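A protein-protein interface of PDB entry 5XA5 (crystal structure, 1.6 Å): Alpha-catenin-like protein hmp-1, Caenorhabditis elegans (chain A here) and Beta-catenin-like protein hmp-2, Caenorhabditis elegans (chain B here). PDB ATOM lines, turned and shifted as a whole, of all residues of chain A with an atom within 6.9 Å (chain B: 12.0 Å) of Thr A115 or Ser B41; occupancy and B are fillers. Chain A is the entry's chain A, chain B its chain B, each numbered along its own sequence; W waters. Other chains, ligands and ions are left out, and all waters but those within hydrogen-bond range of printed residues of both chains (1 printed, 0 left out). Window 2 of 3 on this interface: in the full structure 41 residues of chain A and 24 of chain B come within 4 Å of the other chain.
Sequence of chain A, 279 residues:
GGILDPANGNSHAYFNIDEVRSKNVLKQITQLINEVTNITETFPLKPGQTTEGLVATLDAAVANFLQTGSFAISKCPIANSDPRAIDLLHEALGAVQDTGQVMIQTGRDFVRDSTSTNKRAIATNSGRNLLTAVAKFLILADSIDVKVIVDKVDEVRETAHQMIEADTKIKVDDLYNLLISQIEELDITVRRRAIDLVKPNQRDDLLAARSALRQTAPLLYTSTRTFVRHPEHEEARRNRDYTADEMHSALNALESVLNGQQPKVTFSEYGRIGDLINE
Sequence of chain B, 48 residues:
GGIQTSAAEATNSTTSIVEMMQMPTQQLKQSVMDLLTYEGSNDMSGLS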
ATOM      1  N   PHE A 110      -6.539 -15.191 -26.096  1.00  0.00           N
ATOM      2  CA  PHE A 110      -7.711 -15.836 -25.537  1.00  0.00           C
ATOM      3  C   PHE A 110      -8.106 -15.257 -24.185  1.00  0.00           C
ATOM      4  O   PHE A 110      -9.255 -14.885 -23.997  1.00  0.00           O
ATOM      5  CB  PHE A 110      -7.478 -17.342 -25.413  1.00  0.00           C
ATOM      6  CG  PHE A 110      -8.356 -18.013 -24.392  1.00  0.00           C
ATOM      7  CD1 PHE A 110      -9.738 -17.998 -24.518  1.00  0.00           C
ATOM      8  CD2 PHE A 110      -7.790 -18.681 -23.317  1.00  0.00           C
ATOM      9  CE1 PHE A 110     -10.537 -18.624 -23.572  1.00  0.00           C
ATOM     10  CE2 PHE A 110      -8.575 -19.312 -22.380  1.00  0.00           C
ATOM     11  CZ  PHE A 110      -9.956 -19.277 -22.500  1.00  0.00           C
ATOM     12  N   VAL A 111      -7.170 -15.179 -23.246  1.00  0.00           N
ATOM     13  CA  VAL A 111      -7.520 -14.763 -21.889  1.00  0.00           C
ATOM     14  C   VAL A 111      -7.990 -13.314 -21.860  1.00  0.00           C
ATOM     15  O   VAL A 111      -8.678 -12.891 -20.932  1.00  0.00           O
ATOM     16  CB  VAL A 111      -6.337 -14.924 -20.911  1.00  0.00           C
ATOM     17  CG1 VAL A 111      -5.945 -16.396 -20.784  1.00  0.00           C
ATOM     18  CG2 VAL A 111      -5.153 -14.086 -21.359  1.00  0.00           C
ATOM     19  N   ARG A 112      -7.621 -12.558 -22.885  1.00  0.00           N
ATOM     20  CA  ARG A 112      -8.007 -11.154 -22.963  1.00  0.00           C
ATOM     21  C   ARG A 112      -9.374 -10.978 -23.616  1.00  0.00           C
ATOM     22  O   ARG A 112      -9.973  -9.905 -23.541  1.00  0.00           O
ATOM     23  CB  ARG A 112      -6.948 -10.357 -23.723  1.00  0.00           C
ATOM     24  CG  ARG A 112      -5.731 -10.004 -22.877  1.00  0.00           C
ATOM     25  CD  ARG A 112      -4.679  -9.269 -23.686  1.00  0.00           C
ATOM     26  NE  ARG A 112      -3.575  -8.809 -22.849  1.00  0.00           N
ATOM     27  CZ  ARG A 112      -2.541  -8.104 -23.295  1.00  0.00           C
ATOM     28  NH1 ARG A 112      -2.469  -7.765 -24.577  1.00  0.00           N
ATOM     29  NH2 ARG A 112      -1.585  -7.722 -22.458  1.00  0.00           N
ATOM     30  N   ASP A 113      -9.858 -12.035 -24.258  1.00  0.00           N
ATOM     31  CA  ASP A 113     -11.188 -12.043 -24.862  1.00  0.00           C
ATOM     32  C   ASP A 113     -11.798 -13.409 -24.576  1.00  0.00           C
ATOM     33  O   ASP A 113     -12.113 -14.172 -25.488  1.00  0.00           O
ATOM     34  CB  ASP A 113     -11.104 -11.763 -26.366  1.00  0.00           C
ATOM     35  CG  ASP A 113     -12.469 -11.574 -27.012  1.00  0.00           C
ATOM     36  OD1 ASP A 113     -13.430 -11.218 -26.300  1.00  0.00           O
ATOM     37  OD2 ASP A 113     -12.571 -11.777 -28.243  1.00  0.00           O
ATOM     38  N   SER A 114     -11.960 -13.711 -23.292  1.00  0.00           N
ATOM     39  CA  SER A 114     -12.146 -15.097 -22.865  1.00  0.00           C
ATOM     40  C   SER A 114     -13.521 -15.680 -23.186  1.00  0.00           C
ATOM     41  O   SER A 114     -13.755 -16.865 -22.957  1.00  0.00           O
ATOM     42  CB  SER A 114     -11.868 -15.225 -21.363  1.00  0.00           C
ATOM     43  OG  SER A 114     -12.628 -14.302 -20.607  1.00  0.00           O
ATOM     44  N   THR A 115     -14.427 -14.863 -23.719  1.00  0.00           N
ATOM     45  CA  THR A 115     -15.734 -15.372 -24.130  1.00  0.00           C
ATOM     46  C   THR A 115     -15.745 -15.760 -25.604  1.00  0.00           C
ATOM     47  O   THR A 115     -16.726 -16.312 -26.109  1.00  0.00           O
ATOM     48  CB  THR A 115     -16.857 -14.347 -23.880  1.00  0.00           C
ATOM     49  OG1 THR A 115     -16.724 -13.251 -24.792  1.00  0.00           O
ATOM     50  CG2 THR A 115     -16.815 -13.837 -22.447  1.00  0.00           C
ATOM     51  N   SER A 116     -14.646 -15.478 -26.293  1.00  0.00           N
ATOM     52  CA  SER A 116     -14.534 -15.809 -27.705  1.00  0.00           C
ATOM     53  C   SER A 116     -14.283 -17.301 -27.892  1.00  0.00           C
ATOM     54  O   SER A 116     -13.169 -17.778 -27.675  1.00  0.00           O
ATOM     55  CB  SER A 116     -13.415 -15.000 -28.356  1.00  0.00           C
ATOM     56  OG  SER A 116     -13.078 -15.535 -29.624  1.00  0.00           O
ATOM     57  N   THR A 117     -15.325 -18.032 -28.280  1.00  0.00           N
ATOM     58  CA  THR A 117     -15.215 -19.463 -28.549  1.00  0.00           C
ATOM     59  C   THR A 117     -14.129 -19.754 -29.579  1.00  0.00           C
ATOM     60  O   THR A 117     -13.402 -20.744 -29.474  1.00  0.00           O
ATOM     61  CB  THR A 117     -16.549 -20.047 -29.051  1.00  0.00           C
ATOM     62  OG1 THR A 117     -16.837 -19.532 -30.357  1.00  0.00           O
ATOM     63  CG2 THR A 117     -17.683 -19.698 -28.097  1.00  0.00           C
ATOM     64  N   ASN A 118     -14.013 -18.877 -30.566  1.00  0.00           N
ATOM     65  CA  ASN A 118     -13.034 -19.069 -31.624  1.00  0.00           C
ATOM     66  C   ASN A 118     -11.593 -18.841 -31.158  1.00  0.00           C
ATOM     67  O   ASN A 118     -10.672 -19.529 -31.612  1.00  0.00           O
ATOM     68  CB  ASN A 118     -13.351 -18.151 -32.798  1.00  0.00           C
ATOM     69  CG  ASN A 118     -12.499 -18.454 -34.006  1.00  0.00           C
ATOM     70  OD1 ASN A 118     -12.549 -19.555 -34.554  1.00  0.00           O
ATOM     71  ND2 ASN A 118     -11.697 -17.484 -34.419  1.00  0.00           N
ATOM     72  N   LYS A 119     -11.385 -17.876 -30.265  1.00  0.00           N
ATOM     73  CA  LYS A 119     -10.045 -17.645 -29.729  1.00  0.00           C
ATOM     74  C   LYS A 119      -9.664 -18.749 -28.751  1.00  0.00           C
ATOM     75  O   LYS A 119      -8.484 -19.066 -28.597  1.00  0.00           O
ATOM     76  CB  LYS A 119      -9.939 -16.277 -29.052  1.00  0.00           C
ATOM     77  CG  LYS A 119      -9.755 -15.114 -30.025  1.00  0.00           C
ATOM     78  CD  LYS A 119      -9.823 -13.770 -29.312  1.00  0.00           C
ATOM     79  CE  LYS A 119      -9.734 -12.607 -30.300  1.00  0.00           C
ATOM     80  NZ  LYS A 119     -10.080 -11.329 -29.622  1.00  0.00           N
ATOM     81  N   ARG A 120     -10.661 -19.322 -28.081  1.00  0.00           N
ATOM     82  CA  ARG A 120     -10.405 -20.459 -27.192  1.00  0.00           C
ATOM     83  C   ARG A 120      -9.922 -21.645 -28.012  1.00  0.00           C
ATOM     84  O   ARG A 120      -8.951 -22.321 -27.653  1.00  0.00           O
ATOM     85  CB  ARG A 120     -11.659 -20.836 -26.392  1.00  0.00           C
ATOM     86  CG  ARG A 120     -11.432 -22.032 -25.472  1.00  0.00           C
ATOM     87  CD  ARG A 120     -12.691 -22.439 -24.721  1.00  0.00           C
ATOM     88  NE  ARG A 120     -13.130 -21.420 -23.772  1.00  0.00           N
ATOM     89  CZ  ARG A 120     -12.685 -21.346 -22.523  1.00  0.00           C
ATOM     90  NH1 ARG A 120     -11.767 -22.207 -22.105  1.00  0.00           N
ATOM     91  NH2 ARG A 120     -13.129 -20.402 -21.704  1.00  0.00           N
ATOM     92  N   ASP B  34      -3.957 -25.133 -17.166  1.00  0.00           N
ATOM     93  CA  ASP B  34      -4.540 -24.091 -16.328  1.00  0.00           C
ATOM     94  C   ASP B  34      -5.082 -22.945 -17.170  1.00  0.00           C
ATOM     95  O   ASP B  34      -6.137 -22.378 -16.868  1.00  0.00           O
ATOM     96  CB  ASP B  34      -3.512 -23.536 -15.335  1.00  0.00           C
ATOM     97  CG  ASP B  34      -3.258 -24.459 -14.165  1.00  0.00           C
ATOM     98  OD1 ASP B  34      -3.999 -25.452 -14.008  1.00  0.00           O
ATOM     99  OD2 ASP B  34      -2.317 -24.178 -13.393  1.00  0.00           O
ATOM    100  N   LEU B  35      -4.346 -22.590 -18.217  1.00  0.00           N
ATOM    101  CA  LEU B  35      -4.792 -21.497 -19.079  1.00  0.00           C
ATOM    102  C   LEU B  35      -5.967 -21.947 -19.934  1.00  0.00           C
ATOM    103  O   LEU B  35      -6.924 -21.203 -20.110  1.00  0.00           O
ATOM    104  CB  LEU B  35      -3.651 -20.992 -19.969  1.00  0.00           C
ATOM    105  CG  LEU B  35      -3.917 -19.742 -20.826  1.00  0.00           C
ATOM    106  CD1 LEU B  35      -2.672 -18.882 -20.930  1.00  0.00           C
ATOM    107  CD2 LEU B  35      -4.388 -20.134 -22.214  1.00  0.00           C
ATOM    108  N   LEU B  36      -5.908 -23.163 -20.464  1.00  0.00           N
ATOM    109  CA  LEU B  36      -6.941 -23.585 -21.416  1.00  0.00           C
ATOM    110  C   LEU B  36      -8.247 -23.975 -20.743  1.00  0.00           C
ATOM    111  O   LEU B  36      -9.306 -23.956 -21.378  1.00  0.00           O
ATOM    112  CB  LEU B  36      -6.444 -24.735 -22.290  1.00  0.00           C
ATOM    113  CG  LEU B  36      -5.342 -24.430 -23.305  1.00  0.00           C
ATOM    114  CD1 LEU B  36      -5.014 -25.673 -24.116  1.00  0.00           C
ATOM    115  CD2 LEU B  36      -5.748 -23.282 -24.228  1.00  0.00           C
ATOM    116  N   THR B  37      -8.194 -24.308 -19.460  1.00  0.00           N
ATOM    117  CA  THR B  37      -9.427 -24.659 -18.749  1.00  0.00           C
ATOM    118  C   THR B  37     -10.016 -23.464 -17.973  1.00  0.00           C
ATOM    119  O   THR B  37     -10.945 -23.625 -17.185  1.00  0.00           O
ATOM    120  CB  THR B  37      -9.194 -25.873 -17.792  1.00  0.00           C
ATOM    121  OG1 THR B  37      -8.265 -25.528 -16.758  1.00  0.00           O
ATOM    122  CG2 THR B  37      -8.627 -27.066 -18.563  1.00  0.00           C
ATOM    123  N   TYR B  38      -9.492 -22.264 -18.212  1.00  0.00           N
ATOM    124  CA  TYR B  38     -10.070 -21.058 -17.633  1.00  0.00           C
ATOM    125  C   TYR B  38     -11.433 -20.817 -18.262  1.00  0.00           C
ATOM    126  O   TYR B  38     -11.566 -20.849 -19.479  1.00  0.00           O
ATOM    127  CB  TYR B  38      -9.154 -19.849 -17.847  1.00  0.00           C
ATOM    128  CG  TYR B  38      -9.770 -18.509 -17.510  1.00  0.00           C
ATOM    129  CD1 TYR B  38     -10.377 -18.282 -16.278  1.00  0.00           C
ATOM    130  CD2 TYR B  38      -9.729 -17.464 -18.420  1.00  0.00           C
ATOM    131  CE1 TYR B  38     -10.935 -17.043 -15.971  1.00  0.00           C
ATOM    132  CE2 TYR B  38     -10.286 -16.229 -18.124  1.00  0.00           C
ATOM    133  CZ  TYR B  38     -10.882 -16.027 -16.903  1.00  0.00           C
ATOM    134  OH  TYR B  38     -11.431 -14.797 -16.616  1.00  0.00           O
ATOM    135  N   GLU B  39     -12.440 -20.586 -17.427  1.00  0.00           N
ATOM    136  CA  GLU B  39     -13.821 -20.541 -17.901  1.00  0.00           C
ATOM    137  C   GLU B  39     -14.185 -19.238 -18.599  1.00  0.00           C
ATOM    138  O   GLU B  39     -15.167 -19.178 -19.336  1.00  0.00           O
ATOM    139  CB  GLU B  39     -14.783 -20.762 -16.741  1.00  0.00           C
ATOM    140  CG  GLU B  39     -14.783 -19.653 -15.713  1.00  0.00           C
ATOM    141  CD  GLU B  39     -15.722 -19.960 -14.571  1.00  0.00           C
ATOM    142  OE1 GLU B  39     -16.296 -21.073 -14.573  1.00  0.00           O
ATOM    143  OE2 GLU B  39     -15.885 -19.103 -13.677  1.00  0.00           O
ATOM    144  N   GLY B  40     -13.409 -18.191 -18.352  1.00  0.00           N
ATOM    145  CA  GLY B  40     -13.713 -16.894 -18.924  1.00  0.00           C
ATOM    146  C   GLY B  40     -14.395 -15.972 -17.934  1.00  0.00           C
ATOM    147  O   GLY B  40     -14.550 -16.309 -16.761  1.00  0.00           O
ATOM    148  N   SER B  41     -14.812 -14.806 -18.415  1.00  0.00           N
ATOM    149  CA  SER B  41     -15.347 -13.765 -17.544  1.00  0.00           C
ATOM    150  C   SER B  41     -16.854 -13.886 -17.331  1.00  0.00           C
ATOM    151  O   SER B  41     -17.587 -14.326 -18.217  1.00  0.00           O
ATOM    152  CB  SER B  41     -15.008 -12.390 -18.116  1.00  0.00           C
ATOM    153  OG  SER B  41     -15.344 -12.325 -19.490  1.00  0.00           O
HETATM  154  O   HOH W   1     -10.970 -24.751 -23.255  1.00  0.00           O
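The guanidinium group of Arg A120 lies within hydrogen-bond range of the backbone carbonyl oxygen of Leu B36, 3.1 Å away. The guanidinium group of Arg A120 is in hydrogen-bond range of the backbone carbonyl oxygen of Tyr B38 (2.8 Å). The backbone NH (N) of Ser B41 is in hydrogen-bond range of the side-chain hydroxyl (OG) of Ser A114 (3.1 Å). The guanidinium group (NH2) of Arg A120 lies within hydrogen-bond range of the backbone carbonyl oxygen (O) of Glu B39.
The backbone carbonyl oxygen (O) of Gly B40 sits close to the side-chain hydroxyl (OH) of Tyr B38, at 3.5 Å.
Among the printed residues, merely in contact across the chains: Phe A110 with Leu B35 (3.4 Å), Phe A110 with Tyr B38 (3.8 Å), Val A111 with Leu B35 (3.9 Å), Ser A114 with Tyr B38 (3.7 Å), Ser A114 with Gly B40 (3.3 Å) and Thr A115 with Ser B41 (3.6 Å).
Arg A112 touches none of the printed residues of chain B. Thr A115 touches just one residue of chain B: Ser B41 (3.6 Å). No residue of chain B comes within 4 Å of Ser A116. No residue of chain B comes within 4 Å of Thr A117. Printed residues of chain A within 4 Å of Leu B35: Phe A110 (3.4 Å) and Val A111 (3.9 Å). Of the printed residues of chain A, Gly B40 touches Ser A114. Ser B41 touches just these residues of chain A: Ser A114 (3.1 Å) and Thr A115 (3.6 Å). The nearest residue of chain A that does not touch Ser B41 is Asp A113 (6.3 Å).
Of the 8 printed residues of chain B, 6 touch a printed residue of chain A. Hydrophobic or aromatic side chains of chain B within 4 Å of the printed part of chain A: Leu B35 and Tyr B38. Among the printed residues, 10 pairs touch across the chains. Among the printed residues, no Asp or Glu carboxylate lies within 4 Å of a Lys or Arg side-chain nitrogen of the other chain.
Water W1 bridges the backbone carbonyl oxygen (O) of Leu B36 (2.6 Å) and the guanidinium group (NH1) of Arg A120 (2.9 Å).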
